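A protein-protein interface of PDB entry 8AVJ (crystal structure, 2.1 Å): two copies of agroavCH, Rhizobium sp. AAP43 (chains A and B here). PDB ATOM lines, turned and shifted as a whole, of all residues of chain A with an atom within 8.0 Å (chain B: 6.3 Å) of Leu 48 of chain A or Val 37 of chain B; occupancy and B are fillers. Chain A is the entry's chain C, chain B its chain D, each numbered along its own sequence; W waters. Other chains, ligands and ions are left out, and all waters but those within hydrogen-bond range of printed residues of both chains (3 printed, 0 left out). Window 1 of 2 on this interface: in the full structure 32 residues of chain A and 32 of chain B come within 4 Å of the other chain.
The backbone carbonyl oxygen of Val 21 of chain A is in hydrogen-bond range of the backbone NH of Val 37 of chain A, at 2.7 Å. The side-chain amide oxygen of Asn 69 of chain A lies within hydrogen-bond range of the backbone NH of Ile 71 of chain A (3.0 Å). The backbone carbonyl oxygen (O) of Tyr 35 of chain B lies within hydrogen-bond range of the backbone NH (N) of Thr 23 of chain B, at 3.0 Å. The side-chain hydroxyl of Thr 13 of chain B sits at hydrogen-bond distance from the side-chain hydroxyl of Thr 23 of chain B. The backbone carbonyl oxygen (O) of Val 21 of chain B sits at hydrogen-bond distance from the backbone NH (N) of Val 37 of chain B (2.6 Å). The backbone carbonyl oxygen (O) of Pro 49 of chain A lies within hydrogen-bond range of the side-chain amide nitrogen (ND2) of Asn 69 of chain A (3.0 Å).
Hydrophobic or aromatic side chains of chain B within 4 Å of the printed part of chain A: Val 21, Tyr 35, Val 37, Leu 48 and Pro 49. Of the 18 printed residues of chain A, 5 touch a printed residue of chain B. Hydrophobic or aromatic side chains of chain A that line the printed part of chain B: Tyr 35, Val 37, Leu 48, Pro 49 and Ile 71. Among the printed residues, 9 pairs touch across the chains.
Leu 48 of chain A touches just these residues of chain B: Val 21 and Val 37. Val 37 of chain B touches just one residue of chain A: Leu 48 (3.96 Å). Printed residues of chain A within 4 Å of Thr 23 of chain B: Ile 71. Printed residues of chain B within 4 Å of Tyr 35 of chain A: Leu 48 (3.9 Å) and Pro 49 (3.6 Å). Printed residues of chain A within 4 Å of Thr 13 of chain B: Ile 71 (3.2 Å). Of the printed residues of chain A, Pro 49 of chain B touches Tyr 35 (3.6 Å). Printed residues of chain B within 4 Å of Pro 49 of chain A: Tyr 35. The nearest residue of chain B that does not touch Leu 48 of chain A is Tyr 35 of chain B (4.4 Å). The nearest printed residue of chain A that does not touch Tyr 35 of chain B is Leu 48 of chain A (4.4 Å).
Tyr 35 of chain A touches Leu 48 of chain B, but with the chains exchanged Leu 48 of chain A does not touch Tyr 35 of chain B (4.4 Å). Tyr 35 of chain A touches Pro 49 of chain B, and with the chains exchanged Pro 49 of chain A touches Tyr 35 of chain B. Val 37 of chain A touches Leu 48 of chain B, and with the chains exchanged Leu 48 of chain A touches Val 37 of chain B. Leu 48 of chain A touches Val 21 of chain B, but with the chains exchanged Val 21 of chain A does not touch Leu 48 of chain B (4.2 Å). Of the 9 pairs that touch across the chains among the printed residues, 4 have their exchanged pair printed and touching as well.
Tyr 35 of chain A touches Leu 48 of chain B (OH to CD2, 3.9 Å). Tyr 35 of chain A touches Pro 49 of chain B. Val 37 of chain A touches Leu 48 of chain B. Val 21 of chain B touches Leu 48 of chain A. CD2 of Leu 48 of chain A touches CG2 of Val 37 of chain B (3.96 Å). Tyr 35 of chain B touches Pro 49 of chain A. Ile 71 of chain A touches Thr 13 of chain B. Ile 71 of chain A touches Thr 23 of chain B. Ile 71 of chain A touches Tyr 35 of chain B (CD1 to OH, 3.4 Å).
Water W1 bridges O of Gly 47 of chain A and O of Gly 47 of chain B. Water W3 bridges OD1 of Asn 39 of chain B (2.7 Å) and O of Gly 47 of chain A (2.9 Å). Water W2 lies within hydrogen-bond range of the backbone carbonyl oxygen of Gly 47 of chain B and the backbone carbonyl oxygen of Gly 47 of chain A.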
ATOM      1  N   VAL A  21      10.925 -10.985  -4.921  1.00  0.00           N
ATOM      2  CA  VAL A  21      11.482 -12.324  -5.226  1.00  0.00           C
ATOM      3  C   VAL A  21      10.709 -12.903  -6.405  1.00  0.00           C
ATOM      4  O   VAL A  21       9.464 -12.868  -6.389  1.00  0.00           O
ATOM      5  CB  VAL A  21      11.413 -13.216  -3.975  1.00  0.00           C
ATOM      6  CG1 VAL A  21      11.792 -14.659  -4.278  1.00  0.00           C
ATOM      7  CG2 VAL A  21      12.301 -12.652  -2.872  1.00  0.00           C
ATOM      8  N   TYR A  35       6.448 -17.245 -10.932  1.00  0.00           N
ATOM      9  CA  TYR A  35       5.698 -16.280 -10.123  1.00  0.00           C
ATOM     10  C   TYR A  35       6.680 -15.225  -9.594  1.00  0.00           C
ATOM     11  O   TYR A  35       7.893 -15.452  -9.532  1.00  0.00           O
ATOM     12  CB  TYR A  35       4.859 -17.010  -9.062  1.00  0.00           C
ATOM     13  CG  TYR A  35       5.625 -17.671  -7.943  1.00  0.00           C
ATOM     14  CD1 TYR A  35       6.205 -16.898  -6.954  1.00  0.00           C
ATOM     15  CD2 TYR A  35       5.842 -19.044  -7.899  1.00  0.00           C
ATOM     16  CE1 TYR A  35       6.989 -17.449  -5.958  1.00  0.00           C
ATOM     17  CE2 TYR A  35       6.624 -19.606  -6.896  1.00  0.00           C
ATOM     18  CZ  TYR A  35       7.165 -18.813  -5.902  1.00  0.00           C
ATOM     19  OH  TYR A  35       7.954 -19.283  -4.900  1.00  0.00           O
ATOM     20  N   TYR A  36       6.107 -14.102  -9.197  1.00  0.00           N
ATOM     21  CA  TYR A  36       6.761 -12.887  -8.707  1.00  0.00           C
ATOM     22  C   TYR A  36       6.039 -12.491  -7.443  1.00  0.00           C
ATOM     23  O   TYR A  36       4.801 -12.539  -7.430  1.00  0.00           O
ATOM     24  CB  TYR A  36       6.664 -11.793  -9.756  1.00  0.00           C
ATOM     25  CG  TYR A  36       7.561 -10.632  -9.463  1.00  0.00           C
ATOM     26  CD1 TYR A  36       7.196  -9.646  -8.575  1.00  0.00           C
ATOM     27  CD2 TYR A  36       8.771 -10.509 -10.111  1.00  0.00           C
ATOM     28  CE1 TYR A  36       8.026  -8.551  -8.333  1.00  0.00           C
ATOM     29  CE2 TYR A  36       9.604  -9.436  -9.889  1.00  0.00           C
ATOM     30  CZ  TYR A  36       9.228  -8.464  -8.981  1.00  0.00           C
ATOM     31  OH  TYR A  36      10.062  -7.414  -8.792  1.00  0.00           O
ATOM     32  N   VAL A  37       6.802 -12.221  -6.388  1.00  0.00           N
ATOM     33  CA  VAL A  37       6.288 -11.699  -5.115  1.00  0.00           C
ATOM     34  C   VAL A  37       6.900 -10.316  -4.922  1.00  0.00           C
ATOM     35  O   VAL A  37       8.145 -10.198  -4.783  1.00  0.00           O
ATOM     36  CB  VAL A  37       6.588 -12.630  -3.940  1.00  0.00           C
ATOM     37  CG1 VAL A  37       6.019 -12.055  -2.663  1.00  0.00           C
ATOM     38  CG2 VAL A  37       6.047 -14.043  -4.182  1.00  0.00           C
ATOM     39  N   ASN A  38       6.028  -9.322  -4.897  1.00  0.00           N
ATOM     40  CA  ASN A  38       6.423  -7.903  -4.870  1.00  0.00           C
ATOM     41  C   ASN A  38       6.615  -7.476  -3.403  1.00  0.00           C
ATOM     42  O   ASN A  38       5.734  -7.769  -2.571  1.00  0.00           O
ATOM     43  CB  ASN A  38       5.390  -7.082  -5.630  1.00  0.00           C
ATOM     44  CG  ASN A  38       5.537  -5.602  -5.387  1.00  0.00           C
ATOM     45  OD1 ASN A  38       6.647  -5.067  -5.479  1.00  0.00           O
ATOM     46  ND2 ASN A  38       4.414  -4.953  -5.092  1.00  0.00           N
ATOM     47  N   ASN A  39       7.692  -6.734  -3.136  1.00  0.00           N
ATOM     48  CA  ASN A  39       7.961  -6.076  -1.828  1.00  0.00           C
ATOM     49  C   ASN A  39       8.242  -4.574  -1.989  1.00  0.00           C
ATOM     50  O   ASN A  39       8.758  -3.969  -1.074  1.00  0.00           O
ATOM     51  CB  ASN A  39       9.151  -6.743  -1.165  1.00  0.00           C
ATOM     52  CG  ASN A  39       9.391  -6.268   0.255  1.00  0.00           C
ATOM     53  OD1 ASN A  39      10.489  -5.811   0.628  1.00  0.00           O
ATOM     54  ND2 ASN A  39       8.371  -6.411   1.064  1.00  0.00           N
ATOM     55  N   CYS A  45      -0.437  -4.935  -4.049  1.00  0.00           N
ATOM     56  CA  CYS A  45      -0.159  -6.249  -4.671  1.00  0.00           C
ATOM     57  C   CYS A  45       1.171  -6.796  -4.134  1.00  0.00           C
ATOM     58  O   CYS A  45       2.020  -7.241  -4.948  1.00  0.00           O
ATOM     59  CB  CYS A  45      -0.156  -6.066  -6.188  1.00  0.00           C
ATOM     60  SG  CYS A  45      -1.825  -5.736  -6.824  1.00  0.00           S
ATOM     61  N   ARG A  46       1.364  -6.702  -2.816  1.00  0.00           N
ATOM     62  CA  ARG A  46       2.608  -7.082  -2.120  1.00  0.00           C
ATOM     63  C   ARG A  46       2.399  -8.410  -1.422  1.00  0.00           C
ATOM     64  O   ARG A  46       1.294  -8.631  -1.015  1.00  0.00           O
ATOM     65  CB  ARG A  46       2.959  -6.050  -1.046  1.00  0.00           C
ATOM     66  CG  ARG A  46       3.640  -4.814  -1.601  1.00  0.00           C
ATOM     67  CD  ARG A  46       4.017  -3.776  -0.557  1.00  0.00           C
ATOM     68  NE  ARG A  46       4.934  -4.359   0.405  1.00  0.00           N
ATOM     69  CZ  ARG A  46       5.654  -3.689   1.311  1.00  0.00           C
ATOM     70  NH1 ARG A  46       6.443  -4.344   2.144  1.00  0.00           N
ATOM     71  NH2 ARG A  46       5.606  -2.376   1.382  1.00  0.00           N
ATOM     72  N   GLY A  47       3.442  -9.235  -1.298  1.00  0.00           N
ATOM     73  CA  GLY A  47       3.471 -10.397  -0.386  1.00  0.00           C
ATOM     74  C   GLY A  47       2.793 -11.667  -0.945  1.00  0.00           C
ATOM     75  O   GLY A  47       2.805 -12.686  -0.243  1.00  0.00           O
ATOM     76  N   LEU A  48       2.239 -11.659  -2.154  1.00  0.00           N
ATOM     77  CA  LEU A  48       1.548 -12.860  -2.723  1.00  0.00           C
ATOM     78  C   LEU A  48       2.004 -13.102  -4.157  1.00  0.00           C
ATOM     79  O   LEU A  48       2.338 -12.178  -4.893  1.00  0.00           O
ATOM     80  CB  LEU A  48       0.031 -12.666  -2.628  1.00  0.00           C
ATOM     81  CG  LEU A  48      -0.530 -12.685  -1.197  1.00  0.00           C
ATOM     82  CD1 LEU A  48      -2.012 -12.351  -1.137  1.00  0.00           C
ATOM     83  CD2 LEU A  48      -0.282 -14.016  -0.529  1.00  0.00           C
ATOM     84  N   PRO A  49       2.012 -14.362  -4.621  1.00  0.00           N
ATOM     85  CA  PRO A  49       2.474 -14.652  -5.971  1.00  0.00           C
ATOM     86  C   PRO A  49       1.550 -14.096  -7.059  1.00  0.00           C
ATOM     87  O   PRO A  49       0.345 -14.108  -6.950  1.00  0.00           O
ATOM     88  CB  PRO A  49       2.581 -16.176  -5.998  1.00  0.00           C
ATOM     89  CG  PRO A  49       1.639 -16.646  -4.926  1.00  0.00           C
ATOM     90  CD  PRO A  49       1.609 -15.561  -3.871  1.00  0.00           C
ATOM     91  N   TYR A  50       2.184 -13.575  -8.094  1.00  0.00           N
ATOM     92  CA  TYR A  50       1.570 -13.150  -9.355  1.00  0.00           C
ATOM     93  C   TYR A  50       2.284 -13.965 -10.408  1.00  0.00           C
ATOM     94  O   TYR A  50       3.533 -14.053 -10.287  1.00  0.00           O
ATOM     95  CB  TYR A  50       1.733 -11.633  -9.562  1.00  0.00           C
ATOM     96  CG  TYR A  50       0.797 -10.826  -8.697  1.00  0.00           C
ATOM     97  CD1 TYR A  50       1.082 -10.602  -7.364  1.00  0.00           C
ATOM     98  CD2 TYR A  50      -0.415 -10.353  -9.191  1.00  0.00           C
ATOM     99  CE1 TYR A  50       0.206  -9.902  -6.549  1.00  0.00           C
ATOM    100  CE2 TYR A  50      -1.319  -9.683  -8.380  1.00  0.00           C
ATOM    101  CZ  TYR A  50      -1.009  -9.449  -7.053  1.00  0.00           C
ATOM    102  OH  TYR A  50      -1.892  -8.818  -6.236  1.00  0.00           O
ATOM    103  N   ASP A  51       1.545 -14.463 -11.405  1.00  0.00           N
ATOM    104  CA  ASP A  51       2.092 -15.261 -12.525  1.00  0.00           C
ATOM    105  C   ASP A  51       3.105 -14.433 -13.292  1.00  0.00           C
ATOM    106  O   ASP A  51       2.850 -13.262 -13.503  1.00  0.00           O
ATOM    107  CB  ASP A  51       0.983 -15.700 -13.488  1.00  0.00           C
ATOM    108  CG  ASP A  51       0.145 -16.838 -12.899  1.00  0.00           C
ATOM    109  OD1 ASP A  51       0.617 -17.496 -11.959  1.00  0.00           O
ATOM    110  OD2 ASP A  51      -0.967 -17.062 -13.384  1.00  0.00           O
ATOM    111  N   VAL A  65       4.704  -9.353 -15.728  1.00  0.00           N
ATOM    112  CA  VAL A  65       3.726  -9.640 -14.662  1.00  0.00           C
ATOM    113  C   VAL A  65       2.562  -8.667 -14.845  1.00  0.00           C
ATOM    114  O   VAL A  65       2.757  -7.465 -14.863  1.00  0.00           O
ATOM    115  CB  VAL A  65       4.363  -9.481 -13.278  1.00  0.00           C
ATOM    116  CG1 VAL A  65       3.317  -9.612 -12.182  1.00  0.00           C
ATOM    117  CG2 VAL A  65       5.501 -10.473 -13.072  1.00  0.00           C
ATOM    118  N   TRP A  67      -0.564  -7.353 -12.731  1.00  0.00           N
ATOM    119  CA  TRP A  67      -0.792  -7.261 -11.263  1.00  0.00           C
ATOM    120  C   TRP A  67      -2.264  -7.568 -10.988  1.00  0.00           C
ATOM    121  O   TRP A  67      -2.959  -6.709 -10.433  1.00  0.00           O
ATOM    122  CB  TRP A  67      -0.322  -5.890 -10.743  1.00  0.00           C
ATOM    123  CG  TRP A  67       1.144  -5.699 -10.958  1.00  0.00           C
ATOM    124  CD1 TRP A  67       1.767  -4.933 -11.888  1.00  0.00           C
ATOM    125  CD2 TRP A  67       2.190  -6.418 -10.270  1.00  0.00           C
ATOM    126  NE1 TRP A  67       3.129  -5.089 -11.793  1.00  0.00           N
ATOM    127  CE2 TRP A  67       3.412  -6.001 -10.813  1.00  0.00           C
ATOM    128  CE3 TRP A  67       2.202  -7.306  -9.192  1.00  0.00           C
ATOM    129  CZ2 TRP A  67       4.629  -6.511 -10.382  1.00  0.00           C
ATOM    130  CZ3 TRP A  67       3.410  -7.808  -8.758  1.00  0.00           C
ATOM    131  CH2 TRP A  67       4.606  -7.394  -9.328  1.00  0.00           C
ATOM    132  N   ASN A  69      -4.243 -11.333  -9.638  1.00  0.00           N
ATOM    133  CA  ASN A  69      -4.058 -12.772  -9.355  1.00  0.00           C
ATOM    134  C   ASN A  69      -5.329 -13.323  -8.717  1.00  0.00           C
ATOM    135  O   ASN A  69      -5.242 -14.407  -8.153  1.00  0.00           O
ATOM    136  CB  ASN A  69      -2.848 -13.004  -8.435  1.00  0.00           C
ATOM    137  CG  ASN A  69      -2.986 -12.267  -7.122  1.00  0.00           C
ATOM    138  OD1 ASN A  69      -3.953 -11.548  -6.907  1.00  0.00           O
ATOM    139  ND2 ASN A  69      -2.016 -12.393  -6.238  1.00  0.00           N
ATOM    140  N   ILE A  71      -6.780 -12.088  -6.174  1.00  0.00           N
ATOM    141  CA  ILE A  71      -6.778 -11.646  -4.750  1.00  0.00           C
ATOM    142  C   ILE A  71      -6.690 -10.123  -4.688  1.00  0.00           C
ATOM    143  O   ILE A  71      -7.489  -9.502  -3.936  1.00  0.00           O
ATOM    144  CB  ILE A  71      -5.638 -12.298  -3.952  1.00  0.00           C
ATOM    145  CG1 ILE A  71      -5.718 -13.823  -3.982  1.00  0.00           C
ATOM    146  CG2 ILE A  71      -5.673 -11.761  -2.546  1.00  0.00           C
ATOM    147  CD1 ILE A  71      -4.485 -14.537  -3.455  1.00  0.00           C
ATOM    148  N   ALA A  72      -5.736  -9.532  -5.406  1.00  0.00           N
ATOM    149  CA  ALA A  72      -5.559  -8.066  -5.469  1.00  0.00           C
ATOM    150  C   ALA A  72      -5.199  -7.677  -6.903  1.00  0.00           C
ATOM    151  O   ALA A  72      -4.229  -8.208  -7.455  1.00  0.00           O
ATOM    152  CB  ALA A  72      -4.554  -7.596  -4.438  1.00  0.00           C
ATOM    153  N   THR B  13      -9.371 -16.639  -0.630  1.00  0.00           N
ATOM    154  CA  THR B  13      -8.202 -16.332   0.216  1.00  0.00           C
ATOM    155  C   THR B  13      -8.672 -16.070   1.650  1.00  0.00           C
ATOM    156  O   THR B  13      -9.711 -15.442   1.819  1.00  0.00           O
ATOM    157  CB  THR B  13      -7.388 -15.208  -0.430  1.00  0.00           C
ATOM    158  OG1 THR B  13      -7.037 -15.710  -1.713  1.00  0.00           O
ATOM    159  CG2 THR B  13      -6.132 -14.850   0.338  1.00  0.00           C
ATOM    160  N   GLY B  19      -1.216 -12.668   9.979  1.00  0.00           N
ATOM    161  CA  GLY B  19      -1.046 -12.334   8.550  1.00  0.00           C
ATOM    162  C   GLY B  19      -0.554 -13.484   7.640  1.00  0.00           C
ATOM    163  O   GLY B  19      -0.147 -13.186   6.481  1.00  0.00           O
ATOM    164  N   SER B  20      -0.523 -14.746   8.099  1.00  0.00           N
ATOM    165  CA  SER B  20      -0.260 -15.930   7.229  1.00  0.00           C
ATOM    166  C   SER B  20      -1.455 -16.068   6.303  1.00  0.00           C
ATOM    167  O   SER B  20      -2.555 -15.714   6.734  1.00  0.00           O
ATOM    168  CB  SER B  20      -0.025 -17.161   7.999  1.00  0.00           C
ATOM    169  OG  SER B  20       1.230 -17.106   8.627  1.00  0.00           O
ATOM    170  N   VAL B  21      -1.227 -16.436   5.040  1.00  0.00           N
ATOM    171  CA  VAL B  21      -2.299 -16.428   4.008  1.00  0.00           C
ATOM    172  C   VAL B  21      -2.466 -17.840   3.447  1.00  0.00           C
ATOM    173  O   VAL B  21      -1.434 -18.480   3.146  1.00  0.00           O
ATOM    174  CB  VAL B  21      -2.010 -15.436   2.879  1.00  0.00           C
ATOM    175  CG1 VAL B  21      -3.095 -15.468   1.822  1.00  0.00           C
ATOM    176  CG2 VAL B  21      -1.832 -14.021   3.429  1.00  0.00           C
ATOM    177  N   MET B  22      -3.713 -18.263   3.220  1.00  0.00           N
ATOM    178  CA  MET B  22      -3.982 -19.499   2.433  1.00  0.00           C
ATOM    179  C   MET B  22      -5.004 -19.199   1.345  1.00  0.00           C
ATOM    180  O   MET B  22      -6.027 -18.551   1.615  1.00  0.00           O
ATOM    181  CB  MET B  22      -4.455 -20.657   3.309  1.00  0.00           C
ATOM    182  CG  MET B  22      -5.748 -20.421   3.999  1.00  0.00           C
ATOM    183  SD  MET B  22      -6.207 -21.929   4.894  1.00  0.00           S
ATOM    184  CE  MET B  22      -7.917 -21.529   5.217  1.00  0.00           C
ATOM    185  N   THR B  23      -4.660 -19.569   0.123  1.00  0.00           N
ATOM    186  CA  THR B  23      -5.567 -19.514  -1.036  1.00  0.00           C
ATOM    187  C   THR B  23      -5.931 -20.958  -1.379  1.00  0.00           C
ATOM    188  O   THR B  23      -4.991 -21.780  -1.526  1.00  0.00           O
ATOM    189  CB  THR B  23      -4.908 -18.785  -2.199  1.00  0.00           C
ATOM    190  OG1 THR B  23      -4.545 -17.509  -1.677  1.00  0.00           O
ATOM    191  CG2 THR B  23      -5.837 -18.661  -3.391  1.00  0.00           C
ATOM    192  N   TYR B  35      -2.242 -22.958  -1.966  1.00  0.00           N
ATOM    193  CA  TYR B  35      -0.935 -22.654  -1.342  1.00  0.00           C
ATOM    194  C   TYR B  35      -1.171 -21.862  -0.068  1.00  0.00           C
ATOM    195  O   TYR B  35      -2.239 -21.255   0.141  1.00  0.00           O
ATOM    196  CB  TYR B  35      -0.021 -21.922  -2.328  1.00  0.00           C
ATOM    197  CG  TYR B  35      -0.512 -20.536  -2.656  1.00  0.00           C
ATOM    198  CD1 TYR B  35      -0.334 -19.486  -1.772  1.00  0.00           C
ATOM    199  CD2 TYR B  35      -1.196 -20.283  -3.822  1.00  0.00           C
ATOM    200  CE1 TYR B  35      -0.815 -18.218  -2.045  1.00  0.00           C
ATOM    201  CE2 TYR B  35      -1.645 -19.011  -4.127  1.00  0.00           C
ATOM    202  CZ  TYR B  35      -1.461 -17.984  -3.232  1.00  0.00           C
ATOM    203  OH  TYR B  35      -1.941 -16.752  -3.520  1.00  0.00           O
ATOM    204  N   TYR B  36      -0.162 -21.932   0.774  1.00  0.00           N
ATOM    205  CA  TYR B  36      -0.105 -21.225   2.053  1.00  0.00           C
ATOM    206  C   TYR B  36       1.157 -20.356   2.035  1.00  0.00           C
ATOM    207  O   TYR B  36       2.239 -20.851   1.592  1.00  0.00           O
ATOM    208  CB  TYR B  36      -0.028 -22.275   3.135  1.00  0.00           C
ATOM    209  CG  TYR B  36      -0.228 -21.734   4.510  1.00  0.00           C
ATOM    210  CD1 TYR B  36       0.845 -21.216   5.201  1.00  0.00           C
ATOM    211  CD2 TYR B  36      -1.474 -21.763   5.120  1.00  0.00           C
ATOM    212  CE1 TYR B  36       0.700 -20.797   6.507  1.00  0.00           C
ATOM    213  CE2 TYR B  36      -1.642 -21.281   6.409  1.00  0.00           C
ATOM    214  CZ  TYR B  36      -0.543 -20.800   7.102  1.00  0.00           C
ATOM    215  OH  TYR B  36      -0.629 -20.355   8.394  1.00  0.00           O
ATOM    216  N   VAL B  37       1.028 -19.124   2.505  1.00  0.00           N
ATOM    217  CA  VAL B  37       2.189 -18.209   2.722  1.00  0.00           C
ATOM    218  C   VAL B  37       2.266 -17.944   4.215  1.00  0.00           C
ATOM    219  O   VAL B  37       1.345 -17.312   4.713  1.00  0.00           O
ATOM    220  CB  VAL B  37       2.003 -16.914   1.928  1.00  0.00           C
ATOM    221  CG1 VAL B  37       3.131 -15.907   2.169  1.00  0.00           C
ATOM    222  CG2 VAL B  37       1.854 -17.201   0.457  1.00  0.00           C
ATOM    223  N   ASN B  38       3.321 -18.427   4.851  1.00  0.00           N
ATOM    224  CA  ASN B  38       3.647 -18.234   6.281  1.00  0.00           C
ATOM    225  C   ASN B  38       4.263 -16.832   6.498  1.00  0.00           C
ATOM    226  O   ASN B  38       5.314 -16.529   5.870  1.00  0.00           O
ATOM    227  CB  ASN B  38       4.629 -19.313   6.710  1.00  0.00           C
ATOM    228  CG  ASN B  38       5.144 -19.116   8.117  1.00  0.00           C
ATOM    229  OD1 ASN B  38       4.442 -18.565   8.967  1.00  0.00           O
ATOM    230  ND2 ASN B  38       6.360 -19.572   8.344  1.00  0.00           N
ATOM    231  N   ASN B  39       3.635 -16.018   7.351  1.00  0.00           N
ATOM    232  CA  ASN B  39       4.142 -14.692   7.807  1.00  0.00           C
ATOM    233  C   ASN B  39       4.267 -14.689   9.343  1.00  0.00           C
ATOM    234  O   ASN B  39       4.083 -13.631   9.935  1.00  0.00           O
ATOM    235  CB  ASN B  39       3.247 -13.579   7.243  1.00  0.00           C
ATOM    236  CG  ASN B  39       3.373 -13.420   5.736  1.00  0.00           C
ATOM    237  OD1 ASN B  39       2.394 -13.204   5.017  1.00  0.00           O
ATOM    238  ND2 ASN B  39       4.586 -13.540   5.234  1.00  0.00           N
ATOM    239  N   CYS B  45      10.813 -20.408   6.472  1.00  0.00           N
ATOM    240  CA  CYS B  45       9.891 -20.621   5.311  1.00  0.00           C
ATOM    241  C   CYS B  45       8.800 -19.567   5.293  1.00  0.00           C
ATOM    242  O   CYS B  45       7.584 -19.929   5.106  1.00  0.00           O
ATOM    243  CB  CYS B  45       9.281 -22.013   5.410  1.00  0.00           C
ATOM    244  SG  CYS B  45      10.585 -23.257   5.423  1.00  0.00           S
ATOM    245  N   ARG B  46       9.212 -18.300   5.380  1.00  0.00           N
ATOM    246  CA  ARG B  46       8.279 -17.143   5.376  1.00  0.00           C
ATOM    247  C   ARG B  46       8.224 -16.525   3.988  1.00  0.00           C
ATOM    248  O   ARG B  46       9.269 -16.479   3.340  1.00  0.00           O
ATOM    249  CB  ARG B  46       8.726 -16.088   6.393  1.00  0.00           C
ATOM    250  CG  ARG B  46       8.436 -16.478   7.829  1.00  0.00           C
ATOM    251  CD  ARG B  46       8.820 -15.404   8.821  1.00  0.00           C
ATOM    252  NE  ARG B  46       8.029 -14.196   8.635  1.00  0.00           N
ATOM    253  CZ  ARG B  46       8.082 -13.144   9.454  1.00  0.00           C
ATOM    254  NH1 ARG B  46       7.331 -12.076   9.244  1.00  0.00           N
ATOM    255  NH2 ARG B  46       8.896 -13.165  10.488  1.00  0.00           N
ATOM    256  N   GLY B  47       7.053 -16.025   3.586  1.00  0.00           N
ATOM    257  CA  GLY B  47       6.920 -15.074   2.471  1.00  0.00           C
ATOM    258  C   GLY B  47       6.752 -15.726   1.106  1.00  0.00           C
ATOM    259  O   GLY B  47       6.615 -14.961   0.153  1.00  0.00           O
ATOM    260  N   LEU B  48       6.722 -17.067   0.988  1.00  0.00           N
ATOM    261  CA  LEU B  48       6.654 -17.755  -0.340  1.00  0.00           C
ATOM    262  C   LEU B  48       5.593 -18.866  -0.305  1.00  0.00           C
ATOM    263  O   LEU B  48       5.300 -19.415   0.752  1.00  0.00           O
ATOM    264  CB  LEU B  48       8.039 -18.298  -0.701  1.00  0.00           C
ATOM    265  CG  LEU B  48       9.037 -17.261  -1.218  1.00  0.00           C
ATOM    266  CD1 LEU B  48      10.273 -17.951  -1.744  1.00  0.00           C
ATOM    267  CD2 LEU B  48       8.437 -16.390  -2.329  1.00  0.00           C
ATOM    268  N   PRO B  49       4.904 -19.148  -1.434  1.00  0.00           N
ATOM    269  CA  PRO B  49       3.844 -20.154  -1.456  1.00  0.00           C
ATOM    270  C   PRO B  49       4.450 -21.524  -1.141  1.00  0.00           C
ATOM    271  O   PRO B  49       5.511 -21.818  -1.624  1.00  0.00           O
ATOM    272  CB  PRO B  49       3.264 -20.127  -2.867  1.00  0.00           C
ATOM    273  CG  PRO B  49       4.326 -19.441  -3.705  1.00  0.00           C
ATOM    274  CD  PRO B  49       5.105 -18.538  -2.758  1.00  0.00           C
ATOM    275  N   TYR B  50       3.810 -22.249  -0.237  1.00  0.00           N
ATOM    276  CA  TYR B  50       3.986 -23.706  -0.043  1.00  0.00           C
ATOM    277  C   TYR B  50       2.681 -24.404  -0.434  1.00  0.00           C
ATOM    278  O   TYR B  50       1.625 -23.846  -0.167  1.00  0.00           O
ATOM    279  CB  TYR B  50       4.378 -24.000   1.399  1.00  0.00           C
ATOM    280  CG  TYR B  50       5.788 -23.571   1.708  1.00  0.00           C
ATOM    281  CD1 TYR B  50       6.109 -22.235   1.975  1.00  0.00           C
ATOM    282  CD2 TYR B  50       6.799 -24.508   1.757  1.00  0.00           C
ATOM    283  CE1 TYR B  50       7.422 -21.847   2.225  1.00  0.00           C
ATOM    284  CE2 TYR B  50       8.107 -24.139   2.036  1.00  0.00           C
ATOM    285  CZ  TYR B  50       8.423 -22.802   2.247  1.00  0.00           C
ATOM    286  OH  TYR B  50       9.724 -22.496   2.496  1.00  0.00           O
ATOM    287  N   TRP B  67       6.712 -28.174   4.808  1.00  0.00           N
ATOM    288  CA  TRP B  67       7.508 -26.920   4.709  1.00  0.00           C
ATOM    289  C   TRP B  67       8.738 -27.139   3.834  1.00  0.00           C
ATOM    290  O   TRP B  67       9.838 -26.858   4.291  1.00  0.00           O
ATOM    291  CB  TRP B  67       7.848 -26.417   6.112  1.00  0.00           C
ATOM    292  CG  TRP B  67       6.592 -26.027   6.818  1.00  0.00           C
ATOM    293  CD1 TRP B  67       6.016 -26.708   7.847  1.00  0.00           C
ATOM    294  CD2 TRP B  67       5.696 -24.934   6.508  1.00  0.00           C
ATOM    295  NE1 TRP B  67       4.863 -26.080   8.226  1.00  0.00           N
ATOM    296  CE2 TRP B  67       4.627 -25.010   7.412  1.00  0.00           C
ATOM    297  CE3 TRP B  67       5.677 -23.906   5.563  1.00  0.00           C
ATOM    298  CZ2 TRP B  67       3.574 -24.108   7.418  1.00  0.00           C
ATOM    299  CZ3 TRP B  67       4.637 -23.004   5.565  1.00  0.00           C
ATOM    300  CH2 TRP B  67       3.596 -23.112   6.476  1.00  0.00           C
HETATM  301  O   HOH W   1       4.766 -12.629   1.450  1.00  0.00           O
HETATM  302  O   HOH W   2       4.218 -15.035  -1.199  1.00  0.00           O
HETATM  303  O   HOH W   3       1.675 -12.522   2.458  1.00  0.00           O
